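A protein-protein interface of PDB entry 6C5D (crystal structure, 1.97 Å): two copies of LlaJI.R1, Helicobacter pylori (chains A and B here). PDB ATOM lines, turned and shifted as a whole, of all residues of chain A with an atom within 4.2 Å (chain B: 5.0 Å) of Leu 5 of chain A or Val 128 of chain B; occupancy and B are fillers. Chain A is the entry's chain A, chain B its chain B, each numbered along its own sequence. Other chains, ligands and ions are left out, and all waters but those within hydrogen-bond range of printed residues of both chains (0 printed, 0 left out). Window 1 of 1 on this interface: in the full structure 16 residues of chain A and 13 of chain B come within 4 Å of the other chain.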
ATOM      1  N   VAL A   3      20.898  28.503 -14.628  1.00  0.00           N
ATOM      2  CA  VAL A   3      20.979  28.112 -15.993  1.00  0.00           C
ATOM      3  C   VAL A   3      19.745  27.311 -16.409  1.00  0.00           C
ATOM      4  O   VAL A   3      19.252  26.559 -15.639  1.00  0.00           O
ATOM      5  CB  VAL A   3      22.249  27.273 -16.161  1.00  0.00           C
ATOM      6  CG1 VAL A   3      22.325  26.572 -17.452  1.00  0.00           C
ATOM      7  CG2 VAL A   3      23.481  28.095 -16.021  1.00  0.00           C
ATOM      8  N   TYR A   4      19.248  27.497 -17.605  1.00  0.00           N
ATOM      9  CA  TYR A   4      18.144  26.750 -18.112  1.00  0.00           C
ATOM     10  C   TYR A   4      18.628  26.092 -19.406  1.00  0.00           C
ATOM     11  O   TYR A   4      19.074  26.761 -20.261  1.00  0.00           O
ATOM     12  CB  TYR A   4      16.974  27.669 -18.394  1.00  0.00           C
ATOM     13  CG  TYR A   4      15.827  27.097 -19.144  1.00  0.00           C
ATOM     14  CD1 TYR A   4      15.263  25.923 -18.779  1.00  0.00           C
ATOM     15  CD2 TYR A   4      15.259  27.779 -20.179  1.00  0.00           C
ATOM     16  CE1 TYR A   4      14.190  25.423 -19.443  1.00  0.00           C
ATOM     17  CE2 TYR A   4      14.189  27.279 -20.848  1.00  0.00           C
ATOM     18  CZ  TYR A   4      13.655  26.099 -20.477  1.00  0.00           C
ATOM     19  OH  TYR A   4      12.590  25.615 -21.090  1.00  0.00           O
ATOM     20  N   LEU A   5      18.507  24.788 -19.487  1.00  0.00           N
ATOM     21  CA  LEU A   5      18.947  23.998 -20.620  1.00  0.00           C
ATOM     22  C   LEU A   5      17.697  23.520 -21.324  1.00  0.00           C
ATOM     23  O   LEU A   5      16.848  22.869 -20.702  1.00  0.00           O
ATOM     24  CB  LEU A   5      19.784  22.798 -20.189  1.00  0.00           C
ATOM     25  CG  LEU A   5      20.976  23.001 -19.264  1.00  0.00           C
ATOM     26  CD1 LEU A   5      21.392  21.614 -18.789  1.00  0.00           C
ATOM     27  CD2 LEU A   5      22.124  23.674 -19.998  1.00  0.00           C
ATOM     28  N   ARG A   6      17.577  23.887 -22.588  1.00  0.00           N
ATOM     29  CA  ARG A   6      16.416  23.570 -23.419  1.00  0.00           C
ATOM     30  C   ARG A   6      16.910  22.876 -24.673  1.00  0.00           C
ATOM     31  O   ARG A   6      17.565  23.496 -25.506  1.00  0.00           O
ATOM     32  CB  ARG A   6      15.642  24.828 -23.777  1.00  0.00           C
ATOM     33  CG  ARG A   6      14.356  24.582 -24.547  1.00  0.00           C
ATOM     34  CD  ARG A   6      13.386  23.680 -23.808  1.00  0.00           C
ATOM     35  NE  ARG A   6      12.172  23.618 -24.603  1.00  0.00           N
ATOM     36  CZ  ARG A   6      11.199  24.517 -24.539  1.00  0.00           C
ATOM     37  NH1 ARG A   6      11.255  25.518 -23.667  1.00  0.00           N
ATOM     38  NH2 ARG A   6      10.141  24.393 -25.315  1.00  0.00           N
ATOM     39  N   LYS A   7      16.605  21.592 -24.813  1.00  0.00           N
ATOM     40  CA  LYS A   7      16.996  20.851 -26.007  1.00  0.00           C
ATOM     41  C   LYS A   7      16.080  21.189 -27.189  1.00  0.00           C
ATOM     42  O   LYS A   7      14.852  21.195 -27.060  1.00  0.00           O
ATOM     43  CB  LYS A   7      16.956  19.355 -25.713  1.00  0.00           C
ATOM     44  CG  LYS A   7      17.664  18.520 -26.780  1.00  0.00           C
ATOM     45  CD  LYS A   7      17.655  16.983 -26.449  1.00  0.00           C
ATOM     46  CE  LYS A   7      18.062  16.722 -25.020  1.00  0.00           C
ATOM     47  NZ  LYS A   7      18.336  15.262 -24.760  1.00  0.00           N
ATOM     48  N   LEU A  91      20.036  24.508 -26.064  1.00  0.00           N
ATOM     49  CA  LEU A  91      20.040  25.950 -25.767  1.00  0.00           C
ATOM     50  C   LEU A  91      20.428  26.115 -24.311  1.00  0.00           C
ATOM     51  O   LEU A  91      19.756  25.566 -23.433  1.00  0.00           O
ATOM     52  CB  LEU A  91      18.675  26.583 -26.011  1.00  0.00           C
ATOM     53  CG  LEU A  91      18.205  26.545 -27.476  1.00  0.00           C
ATOM     54  CD1 LEU A  91      16.811  27.218 -27.627  1.00  0.00           C
ATOM     55  CD2 LEU A  91      19.220  27.173 -28.429  1.00  0.00           C
ATOM     56  N   LEU A  92      21.524  26.835 -24.069  1.00  0.00           N
ATOM     57  CA  LEU A  92      22.013  27.134 -22.733  1.00  0.00           C
ATOM     58  C   LEU A  92      21.729  28.602 -22.427  1.00  0.00           C
ATOM     59  O   LEU A  92      22.475  29.481 -22.861  1.00  0.00           O
ATOM     60  CB  LEU A  92      23.506  26.825 -22.609  1.00  0.00           C
ATOM     61  CG  LEU A  92      24.049  26.722 -21.186  1.00  0.00           C
ATOM     62  CD1 LEU A  92      25.461  26.159 -21.164  1.00  0.00           C
ATOM     63  CD2 LEU A  92      24.100  28.042 -20.467  1.00  0.00           C
ATOM     64  N   LEU A 116      26.077  17.985 -20.185  1.00  0.00           N
ATOM     65  CA  LEU A 116      24.839  18.751 -20.073  1.00  0.00           C
ATOM     66  C   LEU A 116      23.627  17.917 -20.484  1.00  0.00           C
ATOM     67  O   LEU A 116      22.568  17.989 -19.844  1.00  0.00           O
ATOM     68  CB  LEU A 116      24.916  20.037 -20.929  1.00  0.00           C
ATOM     69  CG  LEU A 116      26.044  21.017 -20.561  1.00  0.00           C
ATOM     70  CD1 LEU A 116      26.073  22.171 -21.605  1.00  0.00           C
ATOM     71  CD2 LEU A 116      25.932  21.570 -19.140  1.00  0.00           C
ATOM     72  N   LEU A 119      22.524  15.780 -17.565  1.00  0.00           N
ATOM     73  CA  LEU A 119      21.651  16.439 -16.602  1.00  0.00           C
ATOM     74  C   LEU A 119      20.209  16.457 -17.085  1.00  0.00           C
ATOM     75  O   LEU A 119      19.284  16.185 -16.308  1.00  0.00           O
ATOM     76  CB  LEU A 119      22.122  17.876 -16.344  1.00  0.00           C
ATOM     77  CG  LEU A 119      23.515  18.060 -15.764  1.00  0.00           C
ATOM     78  CD1 LEU A 119      23.807  19.537 -15.666  1.00  0.00           C
ATOM     79  CD2 LEU A 119      23.652  17.391 -14.390  1.00  0.00           C
ATOM     80  N   ILE A 120      19.992  16.783 -18.358  1.00  0.00           N
ATOM     81  CA  ILE A 120      18.631  16.825 -18.891  1.00  0.00           C
ATOM     82  C   ILE A 120      17.938  15.477 -18.701  1.00  0.00           C
ATOM     83  O   ILE A 120      16.734  15.422 -18.415  1.00  0.00           O
ATOM     84  CB  ILE A 120      18.647  17.241 -20.373  1.00  0.00           C
ATOM     85  CG1 ILE A 120      19.285  18.615 -20.527  1.00  0.00           C
ATOM     86  CG2 ILE A 120      17.237  17.207 -20.951  1.00  0.00           C
ATOM     87  CD1 ILE A 120      19.376  19.119 -21.971  1.00  0.00           C
ATOM     88  N   MET B   1      13.150  18.852 -14.708  1.00  0.00           N
ATOM     89  CA  MET B   1      14.091  18.402 -13.640  1.00  0.00           C
ATOM     90  C   MET B   1      14.781  19.671 -13.123  1.00  0.00           C
ATOM     91  O   MET B   1      14.966  20.639 -13.877  1.00  0.00           O
ATOM     92  CB  MET B   1      15.105  17.365 -14.188  1.00  0.00           C
ATOM     93  CG  MET B   1      15.602  16.296 -13.162  1.00  0.00           C
ATOM     94  SD  MET B   1      16.642  14.947 -13.846  1.00  0.00           S
ATOM     95  CE  MET B   1      18.332  15.471 -13.472  1.00  0.00           C
ATOM     96  N   LYS B   2      15.130  19.714 -11.844  1.00  0.00           N
ATOM     97  CA  LYS B   2      15.990  20.781 -11.357  1.00  0.00           C
ATOM     98  C   LYS B   2      17.093  20.176 -10.491  1.00  0.00           C
ATOM     99  O   LYS B   2      16.884  19.168  -9.805  1.00  0.00           O
ATOM    100  CB  LYS B   2      15.213  21.884 -10.620  1.00  0.00           C
ATOM    101  CG  LYS B   2      14.109  21.456  -9.696  1.00  0.00           C
ATOM    102  CD  LYS B   2      13.419  22.679  -9.093  1.00  0.00           C
ATOM    103  CE  LYS B   2      12.042  22.329  -8.546  1.00  0.00           C
ATOM    104  NZ  LYS B   2      11.443  23.439  -7.731  1.00  0.00           N
ATOM    105  N   VAL B   3      18.281  20.785 -10.583  1.00  0.00           N
ATOM    106  CA  VAL B   3      19.501  20.341  -9.905  1.00  0.00           C
ATOM    107  C   VAL B   3      20.109  21.549  -9.214  1.00  0.00           C
ATOM    108  O   VAL B   3      20.017  22.682  -9.698  1.00  0.00           O
ATOM    109  CB  VAL B   3      20.512  19.699 -10.896  1.00  0.00           C
ATOM    110  CG1 VAL B   3      21.924  19.846 -10.434  1.00  0.00           C
ATOM    111  CG2 VAL B   3      20.198  18.222 -11.121  1.00  0.00           C
ATOM    112  N   LEU B   5      23.778  22.750  -7.630  1.00  0.00           N
ATOM    113  CA  LEU B   5      25.174  22.488  -7.524  1.00  0.00           C
ATOM    114  C   LEU B   5      25.814  23.359  -6.440  1.00  0.00           C
ATOM    115  O   LEU B   5      25.632  24.545  -6.442  1.00  0.00           O
ATOM    116  CB  LEU B   5      25.852  22.759  -8.838  1.00  0.00           C
ATOM    117  CG  LEU B   5      25.411  22.022 -10.088  1.00  0.00           C
ATOM    118  CD1 LEU B   5      26.194  22.488 -11.271  1.00  0.00           C
ATOM    119  CD2 LEU B   5      25.506  20.549  -9.906  1.00  0.00           C
ATOM    120  N   LEU B 119      30.199  25.465 -15.497  1.00  0.00           N
ATOM    121  CA  LEU B 119      28.932  26.177 -15.286  1.00  0.00           C
ATOM    122  C   LEU B 119      28.927  26.967 -13.986  1.00  0.00           C
ATOM    123  O   LEU B 119      28.406  28.089 -13.935  1.00  0.00           O
ATOM    124  CB  LEU B 119      27.747  25.213 -15.254  1.00  0.00           C
ATOM    125  CG  LEU B 119      27.309  24.410 -16.456  1.00  0.00           C
ATOM    126  CD1 LEU B 119      26.208  23.496 -16.007  1.00  0.00           C
ATOM    127  CD2 LEU B 119      26.837  25.293 -17.641  1.00  0.00           C
ATOM    128  N   LEU B 126      24.678  27.118  -7.824  1.00  0.00           N
ATOM    129  CA  LEU B 126      24.027  27.217  -9.124  1.00  0.00           C
ATOM    130  C   LEU B 126      22.801  26.318  -9.174  1.00  0.00           C
ATOM    131  O   LEU B 126      22.875  25.134  -8.828  1.00  0.00           O
ATOM    132  CB  LEU B 126      24.990  26.817 -10.265  1.00  0.00           C
ATOM    133  CG  LEU B 126      24.437  26.990 -11.682  1.00  0.00           C
ATOM    134  CD1 LEU B 126      24.446  28.447 -12.091  1.00  0.00           C
ATOM    135  CD2 LEU B 126      25.228  26.154 -12.660  1.00  0.00           C
ATOM    136  N   LEU B 127      21.690  26.862  -9.637  1.00  0.00           N
ATOM    137  CA  LEU B 127      20.555  26.047 -10.036  1.00  0.00           C
ATOM    138  C   LEU B 127      20.591  25.792 -11.539  1.00  0.00           C
ATOM    139  O   LEU B 127      20.865  26.706 -12.336  1.00  0.00           O
ATOM    140  CB  LEU B 127      19.248  26.721  -9.642  1.00  0.00           C
ATOM    141  CG  LEU B 127      18.970  26.869  -8.172  1.00  0.00           C
ATOM    142  CD1 LEU B 127      17.558  27.456  -8.013  1.00  0.00           C
ATOM    143  CD2 LEU B 127      19.121  25.516  -7.463  1.00  0.00           C
ATOM    144  N   VAL B 128      20.365  24.571 -11.907  1.00  0.00           N
ATOM    145  CA  VAL B 128      20.247  24.196 -13.296  1.00  0.00           C
ATOM    146  C   VAL B 128      18.791  23.674 -13.539  1.00  0.00           C
ATOM    147  O   VAL B 128      18.481  22.723 -12.916  1.00  0.00           O
ATOM    148  CB  VAL B 128      21.262  23.078 -13.671  1.00  0.00           C
ATOM    149  CG1 VAL B 128      21.128  22.663 -15.110  1.00  0.00           C
ATOM    150  CG2 VAL B 128      22.662  23.487 -13.314  1.00  0.00           C
ATOM    151  N   PHE B 129      17.978  24.272 -14.419  1.00  0.00           N
ATOM    152  CA  PHE B 129      16.608  23.875 -14.783  1.00  0.00           C
ATOM    153  C   PHE B 129      16.638  23.214 -16.216  1.00  0.00           C
ATOM    154  O   PHE B 129      17.454  23.585 -16.991  1.00  0.00           O
ATOM    155  CB  PHE B 129      15.601  25.050 -14.789  1.00  0.00           C
ATOM    156  CG  PHE B 129      15.551  25.819 -13.480  1.00  0.00           C
ATOM    157  CD1 PHE B 129      16.505  26.753 -13.165  1.00  0.00           C
ATOM    158  CD2 PHE B 129      14.612  25.545 -12.526  1.00  0.00           C
ATOM    159  CE1 PHE B 129      16.484  27.411 -11.974  1.00  0.00           C
ATOM    160  CE2 PHE B 129      14.596  26.212 -11.347  1.00  0.00           C
ATOM    161  CZ  PHE B 129      15.533  27.136 -11.064  1.00  0.00           C
ATOM    162  N   SER B 130      15.777  22.229 -16.504  1.00  0.00           N
ATOM    163  CA  SER B 130      15.506  21.648 -17.853  1.00  0.00           C
ATOM    164  C   SER B 130      13.997  21.209 -17.992  1.00  0.00           C
ATOM    165  O   SER B 130      13.306  21.291 -17.022  1.00  0.00           O
ATOM    166  CB  SER B 130      16.467  20.547 -18.166  1.00  0.00           C
ATOM    167  OG  SER B 130      16.761  19.794 -17.037  1.00  0.00           O
ATOM    168  N   GLU B 131      13.555  20.819 -19.184  1.00  0.00           N
ATOM    169  CA  GLU B 131      12.179  20.402 -19.552  1.00  0.00           C
ATOM    170  C   GLU B 131      11.217  21.580 -19.768  1.00  0.00           C
ATOM    171  O   GLU B 131      11.508  22.500 -20.553  1.00  0.00           O
ATOM    172  CB  GLU B 131      11.585  19.229 -18.711  1.00  0.00           C
ATOM    173  CG  GLU B 131      12.200  17.878 -19.052  1.00  0.00           C
ATOM    174  CD  GLU B 131      12.287  17.628 -20.552  1.00  0.00           C
ATOM    175  OE1 GLU B 131      13.338  17.136 -21.024  1.00  0.00           O
ATOM    176  OE2 GLU B 131      11.300  17.948 -21.264  1.00  0.00           O
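O of Leu 127 of chain B lies within hydrogen-bond range of N of Val 3 of chain A.
N of Phe 129 of chain B is in hydrogen-bond range of O of Val 3 of chain A (2.9 Å).
OH of Tyr 4 of chain A lies within hydrogen-bond range of O of Glu 131 of chain B (3.3 Å).
The backbone carbonyl oxygen of Phe 129 of chain B is in hydrogen-bond range of the backbone NH of Leu 5 of chain A (3.0 Å).
NH1 of Arg 6 of chain A lies within hydrogen-bond range of OH of Tyr 4 of chain A, at 2.9 Å.
The backbone NH (N) of Leu 91 of chain A lies within hydrogen-bond range of the backbone carbonyl oxygen (O) of Arg 6 of chain A, at 2.7 Å.
The backbone carbonyl oxygen (O) of Met 1 of chain B sits at hydrogen-bond distance from the backbone NH (N) of Ser 130 of chain B (3.2 Å).
N of Val 128 of chain B sits at hydrogen-bond distance from O of Val 3 of chain B (2.9 Å).
Among the printed residues, merely in contact across the chains: Val 3 of chain A with Val 128 of chain B, Tyr 4 of chain A with Phe 129 of chain B, Leu 5 of chain A with Val 128 of chain B, Leu 5 of chain A with Ser 130 of chain B, Arg 6 of chain A with Glu 131 of chain B, Leu 92 of chain A with Leu 119 of chain B, Leu 116 of chain A with Leu 119 of chain B, Leu 119 of chain A with Met 1 of chain B, Ile 120 of chain A with Ser 130 of chain B and Ile 120 of chain A with Glu 131 of chain B.
Of chain A, only Val 3 and Leu 5 come within 4 Å of Val 128 of chain B.
Of the printed residues of chain A, Ser 130 of chain B touches Leu 5 (3.4 Å) and Ile 120 (3.97 Å).
Printed residues of chain B within 4 Å of Leu 119 of chain A: Met 1.
Of the printed residues of chain A, Phe 129 of chain B touches Val 3, Tyr 4 and Leu 5.
Printed residues of chain B within 4 Å of Arg 6 of chain A: Glu 131.
The nearest residue of chain B that does not touch Leu 5 of chain A is Glu 131 of chain B (4.2 Å).
Of the 10 printed residues of chain A, 8 touch a printed residue of chain B.
Hydrophobic or aromatic side chains of chain B within 4 Å of the printed part of chain A: Met 1, Leu 119, Val 128 and Phe 129.
Among the printed residues, 14 pairs touch across the chains.
3 positions are printed for both chains.
Of the 14 pairs that touch across the chains among the printed residues, none has its exchanged pair printed and touching as well.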
